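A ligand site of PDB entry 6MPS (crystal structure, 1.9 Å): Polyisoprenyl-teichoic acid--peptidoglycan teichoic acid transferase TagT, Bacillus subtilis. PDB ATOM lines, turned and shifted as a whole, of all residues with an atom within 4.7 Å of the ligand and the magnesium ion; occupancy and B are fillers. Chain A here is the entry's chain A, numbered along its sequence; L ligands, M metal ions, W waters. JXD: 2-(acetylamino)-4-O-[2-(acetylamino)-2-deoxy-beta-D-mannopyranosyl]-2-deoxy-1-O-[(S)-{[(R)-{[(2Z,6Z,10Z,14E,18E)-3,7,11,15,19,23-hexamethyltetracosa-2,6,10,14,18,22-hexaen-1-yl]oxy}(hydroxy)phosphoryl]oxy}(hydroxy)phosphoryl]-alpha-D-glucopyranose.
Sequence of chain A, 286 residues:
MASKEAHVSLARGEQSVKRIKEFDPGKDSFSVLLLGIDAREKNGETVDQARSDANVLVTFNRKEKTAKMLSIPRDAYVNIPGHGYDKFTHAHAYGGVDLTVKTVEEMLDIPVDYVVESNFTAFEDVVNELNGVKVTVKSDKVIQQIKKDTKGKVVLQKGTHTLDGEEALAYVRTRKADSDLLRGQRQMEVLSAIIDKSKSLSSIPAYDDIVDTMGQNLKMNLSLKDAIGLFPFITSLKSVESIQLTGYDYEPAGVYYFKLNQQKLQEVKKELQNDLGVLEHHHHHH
An oxygen (O26) of the ligand is in salt-bridge range of the guanidinium group (NH1) of Arg 183 (2.7 Å).
The guanidinium group (NH2) of Arg 173 is in salt-bridge range of an oxygen (O29) of the ligand (2.9 Å).
The guanidinium group (NH2) of Arg 74 lies within salt-bridge range of an oxygen (O26) of the ligand (3.3 Å).
NE of Arg 175 is in salt-bridge range of O26 of the ligand (3.0 Å).
The side-chain carboxylate (OD2) of Asp 53 lies within salt-bridge range of the guanidinium group (NH1) of Arg 74 (2.6 Å).
The backbone NH (N) of Asp 53 is in hydrogen-bond range of the backbone carbonyl oxygen (O) of Gly 36.
The guanidinium group (NH1) of Arg 183 sits at hydrogen-bond distance from the backbone carbonyl oxygen (O) of Arg 173, 2.8 Å away.
O of Val 172 sits close to OE1 of Gln 187, at 3.3 Å.
The backbone carbonyl oxygen (O) of Leu 35 is in hydrogen-bond range of the backbone NH (N) of Ser 118.
O of Ser 118 sits at hydrogen-bond distance from N of Ile 37, at 2.7 Å.
The backbone carbonyl oxygen (O) of Ala 54 is in hydrogen-bond range of the backbone NH (N) of Gly 36, 2.9 Å away.
The backbone NH (N) of Leu 34 sits at hydrogen-bond distance from the backbone carbonyl oxygen (O) of Val 56 (2.7 Å).
Residues that only touch the ligand: Val 32, Leu 34, Leu 35, Gly 36, Ile 37, Phe 60, Ser 118, Asn 119, Phe 120, Phe 123, Val 126, Val 172, Lys 176 and Gln 187.
Hydrophobic or aromatic side chains that line the ligand: Val 32, Leu 34, Phe 60, Phe 120, Phe 123 and Val 126.
20 residues have an atom within 4 Å of the ligand: Val 32, Leu 34, Leu 35, Gly 36, Ile 37, Asp 38, Asp 53, Phe 60, Arg 74, Ser 118, Asn 119, Phe 120, Phe 123, Val 126, Val 172, Arg 173, Arg 175, Lys 176, Arg 183 and Gln 187.
The nearest printed residue that does not touch the ligand is Ala 54 (4.02 Å).
Two residues have an atom within 4 Å of the magnesium ion: Asp 38 and Asp 53.
The magnesium ion is bound by water W3 (2.0 Å), water W1 (2.0 Å), O61 of the ligand (2.0 Å), OD1 of Asp 53 (2.1 Å), O62 of the ligand (2.2 Å) and OD2 of Asp 38 (2.2 Å).
Water W2 lies within hydrogen-bond range of O67 of the ligand, N of Arg 175, OD1 of Asp 149 and N of Lys 176.
Water W4 lies within hydrogen-bond range of NH2 of Arg 74, O24 of the ligand and NH2 of Arg 175.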
ATOM      1  N   VAL A  32      11.855  26.941   9.026  1.00  0.00           N
ATOM      2  CA  VAL A  32      11.629  25.513   9.193  1.00  0.00           C
ATOM      3  C   VAL A  32      10.117  25.287   9.244  1.00  0.00           C
ATOM      4  O   VAL A  32       9.431  25.894  10.061  1.00  0.00           O
ATOM      5  CB  VAL A  32      12.293  24.951  10.467  1.00  0.00           C
ATOM      6  CG1 VAL A  32      12.075  23.452  10.564  1.00  0.00           C
ATOM      7  CG2 VAL A  32      13.786  25.290  10.479  1.00  0.00           C
ATOM      8  N   LEU A  34       7.205  22.731  10.127  1.00  0.00           N
ATOM      9  CA  LEU A  34       6.935  21.541  10.920  1.00  0.00           C
ATOM     10  C   LEU A  34       5.545  21.034  10.582  1.00  0.00           C
ATOM     11  O   LEU A  34       4.561  21.766  10.709  1.00  0.00           O
ATOM     12  CB  LEU A  34       7.037  21.846  12.426  1.00  0.00           C
ATOM     13  CG  LEU A  34       8.382  22.306  12.993  1.00  0.00           C
ATOM     14  CD1 LEU A  34       9.512  21.367  12.603  1.00  0.00           C
ATOM     15  CD2 LEU A  34       8.711  23.737  12.589  1.00  0.00           C
ATOM     16  N   LEU A  35       5.468  19.778  10.150  1.00  0.00           N
ATOM     17  CA  LEU A  35       4.210  19.146   9.772  1.00  0.00           C
ATOM     18  C   LEU A  35       3.951  17.943  10.673  1.00  0.00           C
ATOM     19  O   LEU A  35       4.797  17.048  10.772  1.00  0.00           O
ATOM     20  CB  LEU A  35       4.229  18.714   8.307  1.00  0.00           C
ATOM     21  CG  LEU A  35       4.513  19.831   7.287  1.00  0.00           C
ATOM     22  CD1 LEU A  35       4.553  19.258   5.883  1.00  0.00           C
ATOM     23  CD2 LEU A  35       3.469  20.937   7.384  1.00  0.00           C
ATOM     24  N   GLY A  36       2.790  17.932  11.316  1.00  0.00           N
ATOM     25  CA  GLY A  36       2.388  16.811  12.152  1.00  0.00           C
ATOM     26  C   GLY A  36       1.324  15.965  11.486  1.00  0.00           C
ATOM     27  O   GLY A  36       0.242  16.450  11.160  1.00  0.00           O
ATOM     28  N   ILE A  37       1.634  14.687  11.283  1.00  0.00           N
ATOM     29  CA  ILE A  37       0.763  13.757  10.580  1.00  0.00           C
ATOM     30  C   ILE A  37      -0.023  12.957  11.610  1.00  0.00           C
ATOM     31  O   ILE A  37       0.519  12.588  12.665  1.00  0.00           O
ATOM     32  CB  ILE A  37       1.566  12.821   9.653  1.00  0.00           C
ATOM     33  CG1 ILE A  37       2.658  13.608   8.921  1.00  0.00           C
ATOM     34  CG2 ILE A  37       0.638  12.168   8.666  1.00  0.00           C
ATOM     35  CD1 ILE A  37       2.146  14.781   8.093  1.00  0.00           C
ATOM     36  N   ASP A  38      -1.290  12.666  11.300  1.00  0.00           N
ATOM     37  CA  ASP A  38      -2.192  12.046  12.260  1.00  0.00           C
ATOM     38  C   ASP A  38      -2.259  10.532  12.117  1.00  0.00           C
ATOM     39  O   ASP A  38      -3.319   9.927  12.332  1.00  0.00           O
ATOM     40  CB  ASP A  38      -3.590  12.655  12.132  1.00  0.00           C
ATOM     41  CG  ASP A  38      -4.283  12.289  10.828  1.00  0.00           C
ATOM     42  OD1 ASP A  38      -3.656  11.625   9.975  1.00  0.00           O
ATOM     43  OD2 ASP A  38      -5.463  12.670  10.654  1.00  0.00           O
ATOM     44  N   ASP A  53      -2.264  17.445  10.049  1.00  0.00           N
ATOM     45  CA  ASP A  53      -3.167  18.258  10.851  1.00  0.00           C
ATOM     46  C   ASP A  53      -2.462  19.381  11.611  1.00  0.00           C
ATOM     47  O   ASP A  53      -3.124  20.332  12.028  1.00  0.00           O
ATOM     48  CB  ASP A  53      -3.922  17.374  11.856  1.00  0.00           C
ATOM     49  CG  ASP A  53      -4.962  16.500  11.184  1.00  0.00           C
ATOM     50  OD1 ASP A  53      -5.024  15.287  11.494  1.00  0.00           O
ATOM     51  OD2 ASP A  53      -5.718  17.013  10.321  1.00  0.00           O
ATOM     52  N   ALA A  54      -1.150  19.293  11.789  1.00  0.00           N
ATOM     53  CA  ALA A  54      -0.374  20.351  12.414  1.00  0.00           C
ATOM     54  C   ALA A  54       0.557  20.959  11.369  1.00  0.00           C
ATOM     55  O   ALA A  54       1.239  20.228  10.639  1.00  0.00           O
ATOM     56  CB  ALA A  54       0.432  19.823  13.607  1.00  0.00           C
ATOM     57  N   VAL A  56       3.177  24.236  11.319  1.00  0.00           N
ATOM     58  CA  VAL A  56       3.800  25.347  12.038  1.00  0.00           C
ATOM     59  C   VAL A  56       5.076  25.730  11.305  1.00  0.00           C
ATOM     60  O   VAL A  56       5.991  24.909  11.168  1.00  0.00           O
ATOM     61  CB  VAL A  56       4.099  24.975  13.498  1.00  0.00           C
ATOM     62  CG1 VAL A  56       4.840  26.122  14.202  1.00  0.00           C
ATOM     63  CG2 VAL A  56       2.816  24.642  14.238  1.00  0.00           C
ATOM     64  N   PHE A  60      13.715  31.921  11.852  1.00  0.00           N
ATOM     65  CA  PHE A  60      14.791  32.258  12.782  1.00  0.00           C
ATOM     66  C   PHE A  60      15.572  33.434  12.240  1.00  0.00           C
ATOM     67  O   PHE A  60      16.177  33.346  11.162  1.00  0.00           O
ATOM     68  CB  PHE A  60      15.718  31.061  12.992  1.00  0.00           C
ATOM     69  CG  PHE A  60      15.056  29.877  13.652  1.00  0.00           C
ATOM     70  CD1 PHE A  60      14.946  29.806  15.023  1.00  0.00           C
ATOM     71  CD2 PHE A  60      14.548  28.843  12.888  1.00  0.00           C
ATOM     72  CE1 PHE A  60      14.352  28.720  15.626  1.00  0.00           C
ATOM     73  CE2 PHE A  60      13.945  27.755  13.484  1.00  0.00           C
ATOM     74  CZ  PHE A  60      13.844  27.696  14.856  1.00  0.00           C
ATOM     75  N   ARG A  74      -5.375  24.835   8.987  1.00  0.00           N
ATOM     76  CA  ARG A  74      -5.472  23.760   8.005  1.00  0.00           C
ATOM     77  C   ARG A  74      -6.584  24.008   6.997  1.00  0.00           C
ATOM     78  O   ARG A  74      -6.533  23.463   5.888  1.00  0.00           O
ATOM     79  CB  ARG A  74      -5.659  22.416   8.714  1.00  0.00           C
ATOM     80  CG  ARG A  74      -7.044  22.141   9.261  1.00  0.00           C
ATOM     81  CD  ARG A  74      -7.111  20.737   9.835  1.00  0.00           C
ATOM     82  NE  ARG A  74      -8.361  20.456  10.530  1.00  0.00           N
ATOM     83  CZ  ARG A  74      -8.702  19.277  11.022  1.00  0.00           C
ATOM     84  NH1 ARG A  74      -7.887  18.234  10.896  1.00  0.00           N
ATOM     85  NH2 ARG A  74      -9.861  19.121  11.650  1.00  0.00           N
ATOM     86  N   SER A 118       6.481  14.697  10.975  1.00  0.00           N
ATOM     87  CA  SER A 118       6.470  13.859  12.173  1.00  0.00           C
ATOM     88  C   SER A 118       5.110  13.214  12.339  1.00  0.00           C
ATOM     89  O   SER A 118       4.078  13.841  12.079  1.00  0.00           O
ATOM     90  CB  SER A 118       6.790  14.684  13.415  1.00  0.00           C
ATOM     91  OG  SER A 118       6.767  13.877  14.582  1.00  0.00           O
ATOM     92  N   ASN A 119       5.108  11.963  12.804  1.00  0.00           N
ATOM     93  CA  ASN A 119       3.900  11.284  13.241  1.00  0.00           C
ATOM     94  C   ASN A 119       3.815  11.346  14.765  1.00  0.00           C
ATOM     95  O   ASN A 119       4.662  11.937  15.442  1.00  0.00           O
ATOM     96  CB  ASN A 119       3.872   9.836  12.733  1.00  0.00           C
ATOM     97  CG  ASN A 119       5.041   9.009  13.245  1.00  0.00           C
ATOM     98  OD1 ASN A 119       5.625   9.301  14.296  1.00  0.00           O
ATOM     99  ND2 ASN A 119       5.382   7.969  12.505  1.00  0.00           N
ATOM    100  N   PHE A 120       2.776  10.710  15.319  1.00  0.00           N
ATOM    101  CA  PHE A 120       2.569  10.743  16.760  1.00  0.00           C
ATOM    102  C   PHE A 120       3.759  10.159  17.506  1.00  0.00           C
ATOM    103  O   PHE A 120       4.175  10.690  18.551  1.00  0.00           O
ATOM    104  CB  PHE A 120       1.290   9.982  17.135  1.00  0.00           C
ATOM    105  CG  PHE A 120       0.022  10.591  16.617  1.00  0.00           C
ATOM    106  CD1 PHE A 120      -0.006  11.894  16.136  1.00  0.00           C
ATOM    107  CD2 PHE A 120      -1.144   9.860  16.612  1.00  0.00           C
ATOM    108  CE1 PHE A 120      -1.186  12.445  15.677  1.00  0.00           C
ATOM    109  CE2 PHE A 120      -2.327  10.396  16.145  1.00  0.00           C
ATOM    110  CZ  PHE A 120      -2.347  11.693  15.675  1.00  0.00           C
ATOM    111  N   PHE A 123       6.843  12.467  17.947  1.00  0.00           N
ATOM    112  CA  PHE A 123       6.537  13.526  18.905  1.00  0.00           C
ATOM    113  C   PHE A 123       6.612  12.989  20.331  1.00  0.00           C
ATOM    114  O   PHE A 123       7.282  13.570  21.193  1.00  0.00           O
ATOM    115  CB  PHE A 123       5.163  14.107  18.620  1.00  0.00           C
ATOM    116  CG  PHE A 123       4.751  15.185  19.573  1.00  0.00           C
ATOM    117  CD1 PHE A 123       3.926  14.888  20.648  1.00  0.00           C
ATOM    118  CD2 PHE A 123       5.189  16.483  19.416  1.00  0.00           C
ATOM    119  CE1 PHE A 123       3.542  15.881  21.530  1.00  0.00           C
ATOM    120  CE2 PHE A 123       4.813  17.472  20.290  1.00  0.00           C
ATOM    121  CZ  PHE A 123       3.993  17.171  21.359  1.00  0.00           C
ATOM    122  N   VAL A 126      10.208  12.175  21.350  1.00  0.00           N
ATOM    123  CA  VAL A 126      10.990  13.394  21.567  1.00  0.00           C
ATOM    124  C   VAL A 126      10.673  13.988  22.936  1.00  0.00           C
ATOM    125  O   VAL A 126      11.571  14.330  23.710  1.00  0.00           O
ATOM    126  CB  VAL A 126      10.742  14.407  20.438  1.00  0.00           C
ATOM    127  CG1 VAL A 126      11.249  15.804  20.812  1.00  0.00           C
ATOM    128  CG2 VAL A 126      11.408  13.936  19.157  1.00  0.00           C
ATOM    129  N   ASP A 149     -11.558  13.115  24.723  1.00  0.00           N
ATOM    130  CA  ASP A 149     -10.743  12.690  23.584  1.00  0.00           C
ATOM    131  C   ASP A 149     -10.066  11.357  23.852  1.00  0.00           C
ATOM    132  O   ASP A 149     -10.047  10.475  22.981  1.00  0.00           O
ATOM    133  CB  ASP A 149      -9.695  13.749  23.260  1.00  0.00           C
ATOM    134  CG  ASP A 149     -10.293  15.058  22.764  1.00  0.00           C
ATOM    135  OD1 ASP A 149     -11.430  15.032  22.249  1.00  0.00           O
ATOM    136  OD2 ASP A 149      -9.617  16.101  22.883  1.00  0.00           O
ATOM    137  N   LEU A 169       0.829  15.010  23.569  1.00  0.00           N
ATOM    138  CA  LEU A 169       0.197  14.711  22.297  1.00  0.00           C
ATOM    139  C   LEU A 169      -1.301  14.979  22.344  1.00  0.00           C
ATOM    140  O   LEU A 169      -1.876  15.548  21.406  1.00  0.00           O
ATOM    141  CB  LEU A 169       0.467  13.263  21.890  1.00  0.00           C
ATOM    142  CG  LEU A 169      -0.179  12.826  20.569  1.00  0.00           C
ATOM    143  CD1 LEU A 169       0.432  13.598  19.406  1.00  0.00           C
ATOM    144  CD2 LEU A 169      -0.048  11.327  20.363  1.00  0.00           C
ATOM    145  N   VAL A 172      -1.967  18.770  22.218  1.00  0.00           N
ATOM    146  CA  VAL A 172      -1.849  19.429  20.915  1.00  0.00           C
ATOM    147  C   VAL A 172      -2.840  18.902  19.895  1.00  0.00           C
ATOM    148  O   VAL A 172      -2.907  19.439  18.779  1.00  0.00           O
ATOM    149  CB  VAL A 172      -0.420  19.278  20.339  1.00  0.00           C
ATOM    150  CG1 VAL A 172       0.600  19.891  21.288  1.00  0.00           C
ATOM    151  CG2 VAL A 172      -0.081  17.817  20.050  1.00  0.00           C
ATOM    152  N   ARG A 173      -3.626  17.880  20.233  1.00  0.00           N
ATOM    153  CA  ARG A 173      -4.616  17.319  19.325  1.00  0.00           C
ATOM    154  C   ARG A 173      -6.039  17.800  19.599  1.00  0.00           C
ATOM    155  O   ARG A 173      -6.828  17.924  18.657  1.00  0.00           O
ATOM    156  CB  ARG A 173      -4.590  15.788  19.387  1.00  0.00           C
ATOM    157  CG  ARG A 173      -3.418  15.142  18.677  1.00  0.00           C
ATOM    158  CD  ARG A 173      -3.441  13.627  18.848  1.00  0.00           C
ATOM    159  NE  ARG A 173      -4.537  13.002  18.121  1.00  0.00           N
ATOM    160  CZ  ARG A 173      -4.896  11.729  18.233  1.00  0.00           C
ATOM    161  NH1 ARG A 173      -4.248  10.934  19.077  1.00  0.00           N
ATOM    162  NH2 ARG A 173      -5.908  11.252  17.525  1.00  0.00           N
ATOM    163  N   THR A 174      -6.383  18.068  20.858  1.00  0.00           N
ATOM    164  CA  THR A 174      -7.759  18.375  21.222  1.00  0.00           C
ATOM    165  C   THR A 174      -8.241  19.630  20.493  1.00  0.00           C
ATOM    166  O   THR A 174      -7.471  20.556  20.229  1.00  0.00           O
ATOM    167  CB  THR A 174      -7.885  18.570  22.731  1.00  0.00           C
ATOM    168  OG1 THR A 174      -9.270  18.650  23.092  1.00  0.00           O
ATOM    169  CG2 THR A 174      -7.168  19.848  23.181  1.00  0.00           C
ATOM    170  N   ARG A 175      -9.540  19.653  20.170  1.00  0.00           N
ATOM    171  CA  ARG A 175     -10.136  20.854  19.577  1.00  0.00           C
ATOM    172  C   ARG A 175     -11.651  20.953  19.728  1.00  0.00           C
ATOM    173  O   ARG A 175     -12.224  21.994  19.420  1.00  0.00           O
ATOM    174  CB  ARG A 175      -9.788  20.933  18.094  1.00  0.00           C
ATOM    175  CG  ARG A 175     -10.508  19.908  17.215  1.00  0.00           C
ATOM    176  CD  ARG A 175     -10.357  20.228  15.745  1.00  0.00           C
ATOM    177  NE  ARG A 175     -11.120  19.292  14.921  1.00  0.00           N
ATOM    178  CZ  ARG A 175     -12.440  19.358  14.763  1.00  0.00           C
ATOM    179  NH1 ARG A 175     -13.152  20.288  15.372  1.00  0.00           N
ATOM    180  NH2 ARG A 175     -13.059  18.466  13.988  1.00  0.00           N
ATOM    181  N   LYS A 176     -12.339  19.881  20.143  1.00  0.00           N
ATOM    182  CA  LYS A 176     -13.800  19.955  20.149  1.00  0.00           C
ATOM    183  C   LYS A 176     -14.314  21.004  21.112  1.00  0.00           C
ATOM    184  O   LYS A 176     -15.393  21.583  20.882  1.00  0.00           O
ATOM    185  CB  LYS A 176     -14.395  18.589  20.471  1.00  0.00           C
ATOM    186  CG  LYS A 176     -14.389  17.675  19.275  1.00  0.00           C
ATOM    187  CD  LYS A 176     -15.040  16.336  19.574  1.00  0.00           C
ATOM    188  CE  LYS A 176     -14.196  15.176  19.050  1.00  0.00           C
ATOM    189  NZ  LYS A 176     -15.019  14.187  18.308  1.00  0.00           N
ATOM    190  N   ARG A 183      -6.085  25.249  18.866  1.00  0.00           N
ATOM    191  CA  ARG A 183      -5.204  24.090  18.768  1.00  0.00           C
ATOM    192  C   ARG A 183      -3.839  24.489  18.215  1.00  0.00           C
ATOM    193  O   ARG A 183      -2.809  23.991  18.681  1.00  0.00           O
ATOM    194  CB  ARG A 183      -5.833  23.001  17.894  1.00  0.00           C
ATOM    195  CG  ARG A 183      -4.914  21.811  17.655  1.00  0.00           C
ATOM    196  CD  ARG A 183      -5.680  20.577  17.237  1.00  0.00           C
ATOM    197  NE  ARG A 183      -6.156  20.646  15.856  1.00  0.00           N
ATOM    198  CZ  ARG A 183      -6.853  19.694  15.255  1.00  0.00           C
ATOM    199  NH1 ARG A 183      -7.176  18.588  15.916  1.00  0.00           N
ATOM    200  NH2 ARG A 183      -7.234  19.846  13.988  1.00  0.00           N
ATOM    201  N   GLN A 187      -0.176  24.139  19.948  1.00  0.00           N
ATOM    202  CA  GLN A 187       0.967  23.528  19.279  1.00  0.00           C
ATOM    203  C   GLN A 187       2.201  24.421  19.369  1.00  0.00           C
ATOM    204  O   GLN A 187       3.310  23.939  19.642  1.00  0.00           O
ATOM    205  CB  GLN A 187       0.619  23.238  17.818  1.00  0.00           C
ATOM    206  CG  GLN A 187      -0.256  22.005  17.643  1.00  0.00           C
ATOM    207  CD  GLN A 187      -1.020  21.976  16.321  1.00  0.00           C
ATOM    208  OE1 GLN A 187      -2.007  21.248  16.183  1.00  0.00           O
ATOM    209  NE2 GLN A 187      -0.563  22.755  15.340  1.00  0.00           N
ATOM    210  N   VAL A 190       3.541  24.250  22.955  1.00  0.00           N
ATOM    211  CA  VAL A 190       4.322  23.048  23.256  1.00  0.00           C
ATOM    212  C   VAL A 190       5.640  23.051  22.496  1.00  0.00           C
ATOM    213  O   VAL A 190       6.666  22.604  23.016  1.00  0.00           O
ATOM    214  CB  VAL A 190       3.487  21.793  22.937  1.00  0.00           C
ATOM    215  CG1 VAL A 190       4.349  20.528  23.022  1.00  0.00           C
ATOM    216  CG2 VAL A 190       2.308  21.686  23.893  1.00  0.00           C
ATOM    217  N   LEU A 191       5.635  23.555  21.262  1.00  0.00           N
ATOM    218  CA  LEU A 191       6.867  23.617  20.489  1.00  0.00           C
ATOM    219  C   LEU A 191       7.920  24.466  21.204  1.00  0.00           C
ATOM    220  O   LEU A 191       9.087  24.071  21.283  1.00  0.00           O
ATOM    221  CB  LEU A 191       6.595  24.167  19.096  1.00  0.00           C
ATOM    222  CG  LEU A 191       7.820  24.288  18.174  1.00  0.00           C
ATOM    223  CD1 LEU A 191       8.452  22.925  17.937  1.00  0.00           C
ATOM    224  CD2 LEU A 191       7.430  24.939  16.864  1.00  0.00           C
ATOM    225  N   ILE A 195      11.682  23.416  22.872  1.00  0.00           N
ATOM    226  CA  ILE A 195      12.933  24.155  22.711  1.00  0.00           C
ATOM    227  C   ILE A 195      13.520  24.506  24.074  1.00  0.00           C
ATOM    228  O   ILE A 195      14.718  24.344  24.327  1.00  0.00           O
ATOM    229  CB  ILE A 195      12.696  25.423  21.859  1.00  0.00           C
ATOM    230  CG1 ILE A 195      12.383  25.012  20.414  1.00  0.00           C
ATOM    231  CG2 ILE A 195      13.905  26.359  21.898  1.00  0.00           C
ATOM    232  CD1 ILE A 195      11.783  26.111  19.578  1.00  0.00           C
ATOM    233  N   LEU A 218      10.293  10.335  11.803  1.00  0.00           N
ATOM    234  CA  LEU A 218      10.622  11.740  11.612  1.00  0.00           C
ATOM    235  C   LEU A 218      11.377  11.870  10.287  1.00  0.00           C
ATOM    236  O   LEU A 218      12.488  11.347  10.151  1.00  0.00           O
ATOM    237  CB  LEU A 218      11.470  12.263  12.770  1.00  0.00           C
ATOM    238  CG  LEU A 218      11.519  13.787  12.950  1.00  0.00           C
ATOM    239  CD1 LEU A 218      10.206  14.282  13.514  1.00  0.00           C
ATOM    240  CD2 LEU A 218      12.667  14.188  13.864  1.00  0.00           C
ATOM    241  N   ILE A 234      19.599  27.503  18.138  1.00  0.00           N
ATOM    242  CA  ILE A 234      18.169  27.375  18.417  1.00  0.00           C
ATOM    243  C   ILE A 234      17.907  27.399  19.917  1.00  0.00           C
ATOM    244  O   ILE A 234      16.829  27.834  20.349  1.00  0.00           O
ATOM    245  CB  ILE A 234      17.628  26.104  17.753  1.00  0.00           C
ATOM    246  CG1 ILE A 234      17.479  26.330  16.238  1.00  0.00           C
ATOM    247  CG2 ILE A 234      16.291  25.685  18.359  1.00  0.00           C
ATOM    248  CD1 ILE A 234      17.246  25.060  15.441  1.00  0.00           C
HETATM  249  C10 JXD L   1     -14.129   7.608  13.834  1.00  0.00           C
HETATM  250  C12 JXD L   1     -15.084   8.655  13.177  1.00  0.00           C
HETATM  251  C14 JXD L   1     -14.279   9.959  12.775  1.00  0.00           C
HETATM  252  C16 JXD L   1     -13.868  10.212  10.265  1.00  0.00           C
HETATM  253  C20 JXD L   1     -13.806  13.993  12.385  1.00  0.00           C
HETATM  254  C02 JXD L   1     -11.309  12.852  15.219  1.00  0.00           C
HETATM  255  C03 JXD L   1     -12.578  12.737  14.287  1.00  0.00           C
HETATM  256  C05 JXD L   1     -13.430  10.441  14.049  1.00  0.00           C
HETATM  257  C07 JXD L   1     -13.369   8.260  15.025  1.00  0.00           C
HETATM  258  C08 JXD L   1     -12.358   7.217  15.657  1.00  0.00           C
HETATM  259  C17 JXD L   1     -15.111  11.041   9.983  1.00  0.00           C
HETATM  260  C19 JXD L   1     -12.556  14.005  13.332  1.00  0.00           C
HETATM  261  C23 JXD L   1     -11.160  15.358  14.740  1.00  0.00           C
HETATM  262  C31 JXD L   1      -4.139  14.644  14.926  1.00  0.00           C
HETATM  263  C32 JXD L   1      -4.071  16.143  15.260  1.00  0.00           C
HETATM  264  C33 JXD L   1      -2.995  16.950  15.132  1.00  0.00           C
HETATM  265  C34 JXD L   1      -1.661  16.425  14.621  1.00  0.00           C
HETATM  266  C35 JXD L   1      -0.588  15.967  15.675  1.00  0.00           C
HETATM  267  C36 JXD L   1       0.686  15.281  15.236  1.00  0.00           C
HETATM  268  C37 JXD L   1       1.942  15.478  15.714  1.00  0.00           C
HETATM  269  C38 JXD L   1       2.258  16.484  16.826  1.00  0.00           C
HETATM  270  C39 JXD L   1       2.561  17.975  16.467  1.00  0.00           C
HETATM  271  C40 JXD L   1       2.944  18.957  17.567  1.00  0.00           C
HETATM  272  C41 JXD L   1       3.483  20.189  17.455  1.00  0.00           C
HETATM  273  C42 JXD L   1       3.813  20.841  16.115  1.00  0.00           C
HETATM  274  C43 JXD L   1       5.286  21.033  15.686  1.00  0.00           C
HETATM  275  C44 JXD L   1       6.259  19.921  16.024  1.00  0.00           C
HETATM  276  C45 JXD L   1       6.278  18.766  15.259  1.00  0.00           C
HETATM  277  C46 JXD L   1       7.099  17.512  15.359  1.00  0.00           C
HETATM  278  C47 JXD L   1       8.517  17.292  15.870  1.00  0.00           C
HETATM  279  C48 JXD L   1       9.357  18.553  16.114  1.00  0.00           C
HETATM  280  C49 JXD L   1      10.680  18.422  16.496  1.00  0.00           C
HETATM  281  C50 JXD L   1      11.757  19.446  16.809  1.00  0.00           C
HETATM  282  C51 JXD L   1      12.334  20.441  15.808  1.00  0.00           C
HETATM  283  C52 JXD L   1      12.361  21.890  16.299  1.00  0.00           C
HETATM  284  C53 JXD L   1      12.892  22.816  15.419  1.00  0.00           C
HETATM  285  C54 JXD L   1      13.087  24.279  15.533  1.00  0.00           C
HETATM  286  C55 JXD L   1      13.405  22.344  14.084  1.00  0.00           C
HETATM  287  C56 JXD L   1      11.231  16.995  16.643  1.00  0.00           C
HETATM  288  C57 JXD L   1       5.326  18.668  14.073  1.00  0.00           C
HETATM  289  C58 JXD L   1       3.796  21.012  18.691  1.00  0.00           C
HETATM  290  C59 JXD L   1       3.120  14.700  15.166  1.00  0.00           C
HETATM  291  C60 JXD L   1      -3.078  18.419  15.507  1.00  0.00           C
HETATM  292  C63 JXD L   1     -11.170  14.264  15.900  1.00  0.00           C
HETATM  293  C65 JXD L   1      -9.919  15.046  17.987  1.00  0.00           C
HETATM  294  C66 JXD L   1      -8.685  15.010  18.905  1.00  0.00           C
HETATM  295  N15 JXD L   1     -13.527   9.749  11.535  1.00  0.00           N
HETATM  296  N64 JXD L   1     -10.015  14.271  16.820  1.00  0.00           N
HETATM  297  O01 JXD L   1     -11.497  11.887  16.223  1.00  0.00           O
HETATM  298  O04 JXD L   1     -12.542  11.453  13.649  1.00  0.00           O
HETATM  299  O06 JXD L   1     -12.644   9.364  14.550  1.00  0.00           O
HETATM  300  O09 JXD L   1     -11.488   7.924  16.497  1.00  0.00           O
HETATM  301  O11 JXD L   1     -14.914   6.571  14.362  1.00  0.00           O
HETATM  302  O13 JXD L   1     -15.565   8.045  12.012  1.00  0.00           O
HETATM  303  O18 JXD L   1     -13.143   9.961   9.312  1.00  0.00           O
HETATM  304  O21 JXD L   1     -14.930  14.391  13.127  1.00  0.00           O
HETATM  305  O22 JXD L   1     -12.395  15.190  14.037  1.00  0.00           O
HETATM  306  O24 JXD L   1     -10.180  15.171  13.852  1.00  0.00           O
HETATM  307  O26 JXD L   1      -8.882  17.380  14.248  1.00  0.00           O
HETATM  308  O27 JXD L   1      -7.445  15.320  14.747  1.00  0.00           O
HETATM  309  O29 JXD L   1      -7.459  13.110  16.002  1.00  0.00           O
HETATM  310  O30 JXD L   1      -5.106  13.926  15.554  1.00  0.00           O
HETATM  311  O61 JXD L   1      -6.622  13.280  13.524  1.00  0.00           O
HETATM  312  O62 JXD L   1      -8.219  15.632  12.378  1.00  0.00           O
HETATM  313  O67 JXD L   1     -10.825  15.800  18.325  1.00  0.00           O
HETATM  314  P25 JXD L   1      -8.568  15.999  13.826  1.00  0.00           P
HETATM  315  P28 JXD L   1      -6.762  13.863  14.886  1.00  0.00           P
HETATM  316 MG    MG M   1      -6.803  14.101  11.688  1.00  0.00          MG
HETATM  317  O   HOH W   1      -8.526  13.077  11.443  1.00  0.00           O
HETATM  318  O   HOH W   2     -11.080  17.246  20.436  1.00  0.00           O
HETATM  319  O   HOH W   3      -7.331  14.807   9.911  1.00  0.00           O
HETATM  320  O   HOH W   4     -11.378  16.998  11.507  1.00  0.00           O
